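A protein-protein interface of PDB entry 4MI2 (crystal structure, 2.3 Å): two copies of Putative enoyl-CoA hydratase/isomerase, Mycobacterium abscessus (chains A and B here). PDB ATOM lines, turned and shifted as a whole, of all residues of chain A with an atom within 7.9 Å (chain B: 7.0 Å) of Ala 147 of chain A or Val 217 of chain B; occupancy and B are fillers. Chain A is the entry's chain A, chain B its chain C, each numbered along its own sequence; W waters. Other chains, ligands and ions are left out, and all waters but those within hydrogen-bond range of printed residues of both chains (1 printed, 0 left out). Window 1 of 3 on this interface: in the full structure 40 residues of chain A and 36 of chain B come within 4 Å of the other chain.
The backbone NH of Leu 152 of chain A is in hydrogen-bond range of the side-chain carboxylate of Glu 236 of chain B (3.3 Å). The backbone NH of Ala 147 of chain A sits at hydrogen-bond distance from the side-chain amide oxygen of Gln 240 of chain B, at 3.0 Å. OE1 of Glu 236 of chain B is in hydrogen-bond range of OG of Ser 153 of chain A, 2.6 Å away. The side-chain amide nitrogen (NE2) of Gln 240 of chain B is in hydrogen-bond range of the side-chain carboxylate (OD2) of Asp 149 of chain A, at 2.8 Å. N of Ala 148 of chain A lies within hydrogen-bond range of OE1 of Gln 240 of chain B, 3.2 Å away.
The side-chain hydroxyl (OG1) of Thr 142 of chain A sits at hydrogen-bond distance from the backbone carbonyl oxygen (O) of Phe 169 of chain A (2.6 Å). O of Phe 141 of chain A is in hydrogen-bond range of N of Leu 146 of chain A (2.9 Å).
Gln 240 of chain B touches Met 86 of chain A (O to CG, 3.3 Å). Phe 141 of chain A touches Gln 240 of chain B. Ala 213 of chain B touches Gly 145 of chain A. Gly 145 of chain A touches Leu 243 of chain B (O to CB, 3.7 Å). Leu 146 of chain A touches Ala 213 of chain B (O to CB, 3.4 Å). CG2 of Val 217 of chain B touches O of Ala 147 of chain A, at 3.5 Å. CB of Ala 147 of chain A touches CD1 of Leu 220 of chain B (3.99 Å). Asp 149 of chain A touches Glu 236 of chain B (CA to OE2, 3.4 Å). CD1 of Phe 169 of chain A touches CG2 of Val 217 of chain B, 3.6 Å away. Phe 169 of chain A touches Leu 221 of chain B (CE2 to CD2, 3.9 Å).
Of the printed residues of chain B, Phe 141 of chain A touches Gln 240. Of the printed residues of chain B, Ala 147 of chain A touches Val 217, Leu 220, Gln 240 and Leu 243. Printed residues of chain B within 4 Å of Phe 169 of chain A: Val 217 and Leu 221. Of the printed residues of chain A, Val 217 of chain B touches Ala 147 (3.5 Å) and Phe 169 (3.6 Å). Lys 218 of chain B touches none of the printed residues of chain A. The nearest printed residue of chain A that does not touch Val 217 of chain B is Leu 170 of chain A (4.2 Å).
Of the 18 printed residues of chain A, 12 touch a printed residue of chain B. Among the printed residues, no Asp or Glu carboxylate lies within 4 Å of a Lys or Arg side-chain nitrogen of the other chain.
No position is printed for both chains.
Water W1 lies within hydrogen-bond range of the backbone carbonyl oxygen (O) of Ser 153 of chain A (2.7 Å) and the backbone carbonyl oxygen (O) of Leu 221 of chain B (2.8 Å).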
ATOM      1  N   MET A  86      20.370  -8.846 -28.430  1.00  0.00           N
ATOM      2  CA  MET A  86      19.299  -9.670 -28.964  1.00  0.00           C
ATOM      3  C   MET A  86      18.524  -8.992 -30.095  1.00  0.00           C
ATOM      4  O   MET A  86      17.427  -9.415 -30.421  1.00  0.00           O
ATOM      5  CB  MET A  86      18.336 -10.075 -27.851  1.00  0.00           C
ATOM      6  CG  MET A  86      18.996 -10.581 -26.587  1.00  0.00           C
ATOM      7  SD  MET A  86      20.133 -11.945 -26.840  1.00  0.00           S
ATOM      8  CE  MET A  86      19.180 -13.176 -27.729  1.00  0.00           C
ATOM      9  N   THR A 139      15.387 -27.235 -25.604  1.00  0.00           N
ATOM     10  CA  THR A 139      15.070 -25.814 -25.653  1.00  0.00           C
ATOM     11  C   THR A 139      16.337 -24.965 -25.645  1.00  0.00           C
ATOM     12  O   THR A 139      16.414 -23.968 -26.365  1.00  0.00           O
ATOM     13  CB  THR A 139      14.180 -25.379 -24.475  1.00  0.00           C
ATOM     14  OG1 THR A 139      14.776 -25.797 -23.248  1.00  0.00           O
ATOM     15  CG2 THR A 139      12.815 -25.983 -24.586  1.00  0.00           C
ATOM     16  N   ALA A 140      17.302 -25.342 -24.802  1.00  0.00           N
ATOM     17  CA  ALA A 140      18.634 -24.687 -24.730  1.00  0.00           C
ATOM     18  C   ALA A 140      18.652 -23.291 -24.096  1.00  0.00           C
ATOM     19  O   ALA A 140      19.559 -22.981 -23.317  1.00  0.00           O
ATOM     20  CB  ALA A 140      19.300 -24.643 -26.107  1.00  0.00           C
ATOM     21  N   PHE A 141      17.660 -22.459 -24.406  1.00  0.00           N
ATOM     22  CA  PHE A 141      17.670 -21.046 -23.984  1.00  0.00           C
ATOM     23  C   PHE A 141      17.934 -20.798 -22.489  1.00  0.00           C
ATOM     24  O   PHE A 141      18.724 -19.910 -22.144  1.00  0.00           O
ATOM     25  CB  PHE A 141      16.373 -20.341 -24.390  1.00  0.00           C
ATOM     26  CG  PHE A 141      16.173 -20.254 -25.868  1.00  0.00           C
ATOM     27  CD1 PHE A 141      15.167 -20.979 -26.491  1.00  0.00           C
ATOM     28  CD2 PHE A 141      17.002 -19.453 -26.651  1.00  0.00           C
ATOM     29  CE1 PHE A 141      14.985 -20.910 -27.865  1.00  0.00           C
ATOM     30  CE2 PHE A 141      16.827 -19.387 -28.028  1.00  0.00           C
ATOM     31  CZ  PHE A 141      15.812 -20.115 -28.633  1.00  0.00           C
ATOM     32  N   THR A 142      17.293 -21.562 -21.606  1.00  0.00           N
ATOM     33  CA  THR A 142      17.466 -21.335 -20.158  1.00  0.00           C
ATOM     34  C   THR A 142      18.833 -21.766 -19.648  1.00  0.00           C
ATOM     35  O   THR A 142      19.327 -21.217 -18.660  1.00  0.00           O
ATOM     36  CB  THR A 142      16.377 -22.017 -19.330  1.00  0.00           C
ATOM     37  OG1 THR A 142      16.346 -23.414 -19.637  1.00  0.00           O
ATOM     38  CG2 THR A 142      15.022 -21.391 -19.635  1.00  0.00           C
ATOM     39  N   GLY A 143      19.444 -22.732 -20.337  1.00  0.00           N
ATOM     40  CA  GLY A 143      20.823 -23.123 -20.084  1.00  0.00           C
ATOM     41  C   GLY A 143      21.795 -21.957 -20.122  1.00  0.00           C
ATOM     42  O   GLY A 143      22.758 -21.935 -19.372  1.00  0.00           O
ATOM     43  N   ILE A 144      21.526 -20.976 -20.982  1.00  0.00           N
ATOM     44  CA  ILE A 144      22.373 -19.797 -21.113  1.00  0.00           C
ATOM     45  C   ILE A 144      21.684 -18.537 -20.539  1.00  0.00           C
ATOM     46  O   ILE A 144      22.028 -17.414 -20.880  1.00  0.00           O
ATOM     47  CB  ILE A 144      22.825 -19.635 -22.591  1.00  0.00           C
ATOM     48  CG1 ILE A 144      24.145 -18.862 -22.699  1.00  0.00           C
ATOM     49  CG2 ILE A 144      21.758 -18.979 -23.455  1.00  0.00           C
ATOM     50  CD1 ILE A 144      24.722 -18.882 -24.098  1.00  0.00           C
ATOM     51  N   GLY A 145      20.714 -18.738 -19.649  1.00  0.00           N
ATOM     52  CA  GLY A 145      20.067 -17.630 -18.939  1.00  0.00           C
ATOM     53  C   GLY A 145      19.109 -16.791 -19.758  1.00  0.00           C
ATOM     54  O   GLY A 145      18.826 -15.642 -19.405  1.00  0.00           O
ATOM     55  N   LEU A 146      18.613 -17.358 -20.858  1.00  0.00           N
ATOM     56  CA  LEU A 146      17.583 -16.725 -21.685  1.00  0.00           C
ATOM     57  C   LEU A 146      16.295 -17.538 -21.545  1.00  0.00           C
ATOM     58  O   LEU A 146      16.272 -18.534 -20.829  1.00  0.00           O
ATOM     59  CB  LEU A 146      18.040 -16.665 -23.139  1.00  0.00           C
ATOM     60  CG  LEU A 146      19.358 -15.931 -23.394  1.00  0.00           C
ATOM     61  CD1 LEU A 146      19.725 -15.991 -24.873  1.00  0.00           C
ATOM     62  CD2 LEU A 146      19.288 -14.482 -22.918  1.00  0.00           C
ATOM     63  N   ALA A 147      15.228 -17.118 -22.217  1.00  0.00           N
ATOM     64  CA  ALA A 147      13.911 -17.743 -22.067  1.00  0.00           C
ATOM     65  C   ALA A 147      13.500 -18.517 -23.322  1.00  0.00           C
ATOM     66  O   ALA A 147      13.465 -19.757 -23.314  1.00  0.00           O
ATOM     67  CB  ALA A 147      12.872 -16.681 -21.741  1.00  0.00           C
ATOM     68  N   ALA A 148      13.186 -17.787 -24.395  1.00  0.00           N
ATOM     69  CA  ALA A 148      12.681 -18.392 -25.627  1.00  0.00           C
ATOM     70  C   ALA A 148      12.640 -17.400 -26.774  1.00  0.00           C
ATOM     71  O   ALA A 148      12.387 -16.209 -26.576  1.00  0.00           O
ATOM     72  CB  ALA A 148      11.289 -18.975 -25.408  1.00  0.00           C
ATOM     73  N   ASP A 149      12.903 -17.904 -27.976  1.00  0.00           N
ATOM     74  CA  ASP A 149      12.607 -17.176 -29.203  1.00  0.00           C
ATOM     75  C   ASP A 149      12.367 -18.197 -30.332  1.00  0.00           C
ATOM     76  O   ASP A 149      12.291 -19.392 -30.065  1.00  0.00           O
ATOM     77  CB  ASP A 149      13.698 -16.136 -29.516  1.00  0.00           C
ATOM     78  CG  ASP A 149      15.067 -16.751 -29.751  1.00  0.00           C
ATOM     79  OD1 ASP A 149      15.201 -17.615 -30.659  1.00  0.00           O
ATOM     80  OD2 ASP A 149      16.019 -16.337 -29.045  1.00  0.00           O
ATOM     81  N   LEU A 152       9.271 -20.784 -30.085  1.00  0.00           N
ATOM     82  CA  LEU A 152       9.353 -22.028 -29.325  1.00  0.00           C
ATOM     83  C   LEU A 152       8.449 -22.035 -28.096  1.00  0.00           C
ATOM     84  O   LEU A 152       7.982 -23.100 -27.671  1.00  0.00           O
ATOM     85  CB  LEU A 152      10.799 -22.292 -28.909  1.00  0.00           C
ATOM     86  CG  LEU A 152      11.096 -23.719 -28.471  1.00  0.00           C
ATOM     87  CD1 LEU A 152      10.859 -24.733 -29.587  1.00  0.00           C
ATOM     88  CD2 LEU A 152      12.535 -23.771 -27.986  1.00  0.00           C
ATOM     89  N   SER A 153       8.186 -20.846 -27.548  1.00  0.00           N
ATOM     90  CA  SER A 153       7.302 -20.701 -26.400  1.00  0.00           C
ATOM     91  C   SER A 153       5.835 -20.988 -26.750  1.00  0.00           C
ATOM     92  O   SER A 153       5.027 -21.146 -25.855  1.00  0.00           O
ATOM     93  CB  SER A 153       7.451 -19.308 -25.766  1.00  0.00           C
ATOM     94  OG  SER A 153       6.886 -18.282 -26.571  1.00  0.00           O
ATOM     95  N   ALA A 165       6.430 -29.319 -22.072  1.00  0.00           N
ATOM     96  CA  ALA A 165       7.117 -28.124 -22.567  1.00  0.00           C
ATOM     97  C   ALA A 165       7.770 -27.349 -21.417  1.00  0.00           C
ATOM     98  O   ALA A 165       8.951 -26.979 -21.488  1.00  0.00           O
ATOM     99  CB  ALA A 165       6.135 -27.233 -23.323  1.00  0.00           C
ATOM    100  N   THR A 166       7.000 -27.142 -20.350  1.00  0.00           N
ATOM    101  CA  THR A 166       7.477 -26.448 -19.170  1.00  0.00           C
ATOM    102  C   THR A 166       8.690 -27.173 -18.589  1.00  0.00           C
ATOM    103  O   THR A 166       9.719 -26.550 -18.317  1.00  0.00           O
ATOM    104  CB  THR A 166       6.362 -26.339 -18.100  1.00  0.00           C
ATOM    105  OG1 THR A 166       5.256 -25.607 -18.636  1.00  0.00           O
ATOM    106  CG2 THR A 166       6.856 -25.629 -16.857  1.00  0.00           C
ATOM    107  N   PHE A 169      11.839 -26.661 -20.644  1.00  0.00           N
ATOM    108  CA  PHE A 169      12.350 -25.294 -20.459  1.00  0.00           C
ATOM    109  C   PHE A 169      13.004 -25.084 -19.088  1.00  0.00           C
ATOM    110  O   PHE A 169      14.074 -24.475 -18.999  1.00  0.00           O
ATOM    111  CB  PHE A 169      11.228 -24.246 -20.638  1.00  0.00           C
ATOM    112  CG  PHE A 169      11.030 -23.785 -22.059  1.00  0.00           C
ATOM    113  CD1 PHE A 169      12.022 -23.064 -22.716  1.00  0.00           C
ATOM    114  CD2 PHE A 169       9.837 -24.038 -22.731  1.00  0.00           C
ATOM    115  CE1 PHE A 169      11.835 -22.624 -24.022  1.00  0.00           C
ATOM    116  CE2 PHE A 169       9.644 -23.606 -24.038  1.00  0.00           C
ATOM    117  CZ  PHE A 169      10.644 -22.894 -24.681  1.00  0.00           C
ATOM    118  N   LEU A 170      12.351 -25.563 -18.028  1.00  0.00           N
ATOM    119  CA  LEU A 170      12.863 -25.396 -16.662  1.00  0.00           C
ATOM    120  C   LEU A 170      14.010 -26.340 -16.297  1.00  0.00           C
ATOM    121  O   LEU A 170      15.007 -25.909 -15.721  1.00  0.00           O
ATOM    122  CB  LEU A 170      11.732 -25.554 -15.641  1.00  0.00           C
ATOM    123  CG  LEU A 170      10.595 -24.553 -15.807  1.00  0.00           C
ATOM    124  CD1 LEU A 170       9.621 -24.691 -14.656  1.00  0.00           C
ATOM    125  CD2 LEU A 170      11.127 -23.133 -15.910  1.00  0.00           C
ATOM    126  N   ALA B 212      15.548 -15.204 -13.175  1.00  0.00           N
ATOM    127  CA  ALA B 212      14.900 -14.195 -14.023  1.00  0.00           C
ATOM    128  C   ALA B 212      14.436 -14.815 -15.358  1.00  0.00           C
ATOM    129  O   ALA B 212      13.351 -14.512 -15.840  1.00  0.00           O
ATOM    130  CB  ALA B 212      15.812 -12.996 -14.261  1.00  0.00           C
ATOM    131  N   ALA B 213      15.258 -15.698 -15.925  1.00  0.00           N
ATOM    132  CA  ALA B 213      14.903 -16.405 -17.165  1.00  0.00           C
ATOM    133  C   ALA B 213      13.719 -17.345 -16.952  1.00  0.00           C
ATOM    134  O   ALA B 213      12.809 -17.396 -17.777  1.00  0.00           O
ATOM    135  CB  ALA B 213      16.104 -17.169 -17.719  1.00  0.00           C
ATOM    136  N   PHE B 214      13.728 -18.073 -15.844  1.00  0.00           N
ATOM    137  CA  PHE B 214      12.606 -18.972 -15.504  1.00  0.00           C
ATOM    138  C   PHE B 214      11.267 -18.217 -15.379  1.00  0.00           C
ATOM    139  O   PHE B 214      10.245 -18.676 -15.892  1.00  0.00           O
ATOM    140  CB  PHE B 214      12.874 -19.745 -14.195  1.00  0.00           C
ATOM    141  CG  PHE B 214      13.901 -20.854 -14.304  1.00  0.00           C
ATOM    142  CD1 PHE B 214      14.609 -21.250 -13.170  1.00  0.00           C
ATOM    143  CD2 PHE B 214      14.153 -21.517 -15.499  1.00  0.00           C
ATOM    144  CE1 PHE B 214      15.541 -22.276 -13.232  1.00  0.00           C
ATOM    145  CE2 PHE B 214      15.079 -22.542 -15.564  1.00  0.00           C
ATOM    146  CZ  PHE B 214      15.778 -22.919 -14.429  1.00  0.00           C
ATOM    147  N   SER B 215      11.283 -17.080 -14.685  1.00  0.00           N
ATOM    148  CA  SER B 215      10.100 -16.209 -14.578  1.00  0.00           C
ATOM    149  C   SER B 215       9.632 -15.679 -15.931  1.00  0.00           C
ATOM    150  O   SER B 215       8.426 -15.608 -16.179  1.00  0.00           O
ATOM    151  CB  SER B 215      10.377 -15.015 -13.645  1.00  0.00           C
ATOM    152  OG  SER B 215      10.846 -15.476 -12.387  1.00  0.00           O
ATOM    153  N   GLU B 216      10.576 -15.300 -16.794  1.00  0.00           N
ATOM    154  CA  GLU B 216      10.233 -14.822 -18.145  1.00  0.00           C
ATOM    155  C   GLU B 216       9.593 -15.918 -19.002  1.00  0.00           C
ATOM    156  O   GLU B 216       8.532 -15.701 -19.615  1.00  0.00           O
ATOM    157  CB  GLU B 216      11.473 -14.267 -18.860  1.00  0.00           C
ATOM    158  CG  GLU B 216      11.967 -12.936 -18.306  1.00  0.00           C
ATOM    159  CD  GLU B 216      11.216 -11.726 -18.838  1.00  0.00           C
ATOM    160  OE1 GLU B 216      10.225 -11.897 -19.589  1.00  0.00           O
ATOM    161  OE2 GLU B 216      11.630 -10.581 -18.515  1.00  0.00           O
ATOM    162  N   VAL B 217      10.222 -17.093 -19.049  1.00  0.00           N
ATOM    163  CA  VAL B 217       9.746 -18.162 -19.933  1.00  0.00           C
ATOM    164  C   VAL B 217       8.389 -18.733 -19.467  1.00  0.00           C
ATOM    165  O   VAL B 217       7.524 -19.064 -20.282  1.00  0.00           O
ATOM    166  CB  VAL B 217      10.794 -19.282 -20.111  1.00  0.00           C
ATOM    167  CG1 VAL B 217      10.797 -20.241 -18.927  1.00  0.00           C
ATOM    168  CG2 VAL B 217      10.524 -20.046 -21.401  1.00  0.00           C
ATOM    169  N   LYS B 218       8.202 -18.813 -18.156  1.00  0.00           N
ATOM    170  CA  LYS B 218       6.921 -19.225 -17.599  1.00  0.00           C
ATOM    171  C   LYS B 218       5.792 -18.266 -18.029  1.00  0.00           C
ATOM    172  O   LYS B 218       4.700 -18.711 -18.398  1.00  0.00           O
ATOM    173  CB  LYS B 218       7.041 -19.341 -16.079  1.00  0.00           C
ATOM    174  CG  LYS B 218       5.775 -19.694 -15.327  1.00  0.00           C
ATOM    175  CD  LYS B 218       6.132 -20.235 -13.946  1.00  0.00           C
ATOM    176  CE  LYS B 218       5.004 -20.104 -12.950  1.00  0.00           C
ATOM    177  NZ  LYS B 218       5.337 -20.739 -11.653  1.00  0.00           N
ATOM    178  N   GLU B 219       6.071 -16.965 -18.021  1.00  0.00           N
ATOM    179  CA  GLU B 219       5.104 -15.958 -18.475  1.00  0.00           C
ATOM    180  C   GLU B 219       4.874 -16.055 -20.000  1.00  0.00           C
ATOM    181  O   GLU B 219       3.739 -15.927 -20.477  1.00  0.00           O
ATOM    182  CB  GLU B 219       5.575 -14.553 -18.029  1.00  0.00           C
ATOM    183  CG  GLU B 219       4.656 -13.367 -18.354  1.00  0.00           C
ATOM    184  CD  GLU B 219       3.278 -13.429 -17.692  1.00  0.00           C
ATOM    185  OE1 GLU B 219       3.040 -14.292 -16.824  1.00  0.00           O
ATOM    186  OE2 GLU B 219       2.402 -12.616 -18.067  1.00  0.00           O
ATOM    187  N   LEU B 220       5.939 -16.313 -20.761  1.00  0.00           N
ATOM    188  CA  LEU B 220       5.812 -16.511 -22.205  1.00  0.00           C
ATOM    189  C   LEU B 220       4.933 -17.715 -22.525  1.00  0.00           C
ATOM    190  O   LEU B 220       4.011 -17.611 -23.331  1.00  0.00           O
ATOM    191  CB  LEU B 220       7.173 -16.681 -22.879  1.00  0.00           C
ATOM    192  CG  LEU B 220       8.042 -15.432 -22.974  1.00  0.00           C
ATOM    193  CD1 LEU B 220       9.414 -15.810 -23.521  1.00  0.00           C
ATOM    194  CD2 LEU B 220       7.377 -14.367 -23.832  1.00  0.00           C
ATOM    195  N   LEU B 221       5.219 -18.848 -21.892  1.00  0.00           N
ATOM    196  CA  LEU B 221       4.403 -20.059 -22.073  1.00  0.00           C
ATOM    197  C   LEU B 221       2.918 -19.807 -21.789  1.00  0.00           C
ATOM    198  O   LEU B 221       2.052 -20.208 -22.559  1.00  0.00           O
ATOM    199  CB  LEU B 221       4.923 -21.192 -21.183  1.00  0.00           C
ATOM    200  CG  LEU B 221       6.251 -21.831 -21.590  1.00  0.00           C
ATOM    201  CD1 LEU B 221       6.839 -22.642 -20.442  1.00  0.00           C
ATOM    202  CD2 LEU B 221       6.079 -22.712 -22.816  1.00  0.00           C
ATOM    203  N   ARG B 222       2.627 -19.118 -20.694  1.00  0.00           N
ATOM    204  CA  ARG B 222       1.238 -18.775 -20.366  1.00  0.00           C
ATOM    205  C   ARG B 222       0.590 -17.817 -21.351  1.00  0.00           C
ATOM    206  O   ARG B 222      -0.554 -18.021 -21.733  1.00  0.00           O
ATOM    207  CB  ARG B 222       1.139 -18.208 -18.956  1.00  0.00           C
ATOM    208  CG  ARG B 222       1.381 -19.282 -17.914  1.00  0.00           C
ATOM    209  CD  ARG B 222       1.478 -18.698 -16.524  1.00  0.00           C
ATOM    210  NE  ARG B 222       1.475 -19.743 -15.508  1.00  0.00           N
ATOM    211  CZ  ARG B 222       1.596 -19.523 -14.203  1.00  0.00           C
ATOM    212  NH1 ARG B 222       1.733 -18.281 -13.724  1.00  0.00           N
ATOM    213  NH2 ARG B 222       1.576 -20.553 -13.369  1.00  0.00           N
ATOM    214  N   ARG B 223       1.304 -16.770 -21.747  1.00  0.00           N
ATOM    215  CA  ARG B 223       0.723 -15.750 -22.623  1.00  0.00           C
ATOM    216  C   ARG B 223       0.623 -16.199 -24.063  1.00  0.00           C
ATOM    217  O   ARG B 223      -0.238 -15.726 -24.793  1.00  0.00           O
ATOM    218  CB  ARG B 223       1.552 -14.473 -22.587  1.00  0.00           C
ATOM    219  CG  ARG B 223       1.500 -13.727 -21.274  1.00  0.00           C
ATOM    220  CD  ARG B 223       2.349 -12.467 -21.384  1.00  0.00           C
ATOM    221  NE  ARG B 223       1.683 -11.404 -22.144  1.00  0.00           N
ATOM    222  CZ  ARG B 223       2.297 -10.331 -22.635  1.00  0.00           C
ATOM    223  NH1 ARG B 223       3.611 -10.165 -22.472  1.00  0.00           N
ATOM    224  NH2 ARG B 223       1.596  -9.419 -23.303  1.00  0.00           N
ATOM    225  N   GLU B 236       8.528 -12.716 -27.348  1.00  0.00           N
ATOM    226  CA  GLU B 236       9.800 -13.421 -27.257  1.00  0.00           C
ATOM    227  C   GLU B 236      10.987 -12.464 -27.426  1.00  0.00           C
ATOM    228  O   GLU B 236      11.907 -12.481 -26.614  1.00  0.00           O
ATOM    229  CB  GLU B 236       9.872 -14.571 -28.276  1.00  0.00           C
ATOM    230  CG  GLU B 236       9.023 -15.768 -27.880  1.00  0.00           C
ATOM    231  CD  GLU B 236       8.990 -16.854 -28.930  1.00  0.00           C
ATOM    232  OE1 GLU B 236       8.548 -17.969 -28.591  1.00  0.00           O
ATOM    233  OE2 GLU B 236       9.410 -16.603 -30.083  1.00  0.00           O
ATOM    234  N   ALA B 239      11.426 -10.293 -24.239  1.00  0.00           N
ATOM    235  CA  ALA B 239      11.911 -11.096 -23.124  1.00  0.00           C
ATOM    236  C   ALA B 239      13.392 -11.412 -23.261  1.00  0.00           C
ATOM    237  O   ALA B 239      14.143 -11.294 -22.294  1.00  0.00           O
ATOM    238  CB  ALA B 239      11.112 -12.379 -23.003  1.00  0.00           C
ATOM    239  N   GLN B 240      13.809 -11.817 -24.456  1.00  0.00           N
ATOM    240  CA  GLN B 240      15.217 -12.094 -24.710  1.00  0.00           C
ATOM    241  C   GLN B 240      16.060 -10.834 -24.488  1.00  0.00           C
ATOM    242  O   GLN B 240      17.117 -10.908 -23.863  1.00  0.00           O
ATOM    243  CB  GLN B 240      15.437 -12.636 -26.130  1.00  0.00           C
ATOM    244  CG  GLN B 240      14.725 -13.943 -26.460  1.00  0.00           C
ATOM    245  CD  GLN B 240      15.180 -15.114 -25.606  1.00  0.00           C
ATOM    246  OE1 GLN B 240      15.001 -15.127 -24.389  1.00  0.00           O
ATOM    247  NE2 GLN B 240      15.758 -16.112 -26.246  1.00  0.00           N
ATOM    248  N   LEU B 243      16.576 -10.165 -20.814  1.00  0.00           N
ATOM    249  CA  LEU B 243      17.511 -11.141 -20.255  1.00  0.00           C
ATOM    250  C   LEU B 243      18.931 -11.020 -20.797  1.00  0.00           C
ATOM    251  O   LEU B 243      19.878 -11.345 -20.088  1.00  0.00           O
ATOM    252  CB  LEU B 243      16.996 -12.567 -20.456  1.00  0.00           C
ATOM    253  CG  LEU B 243      15.683 -12.849 -19.709  1.00  0.00           C
ATOM    254  CD1 LEU B 243      15.047 -14.138 -20.209  1.00  0.00           C
ATOM    255  CD2 LEU B 243      15.910 -12.899 -18.208  1.00  0.00           C
HETATM  256  O   HOH W   1       2.466 -21.319 -25.086  1.00  0.00           O
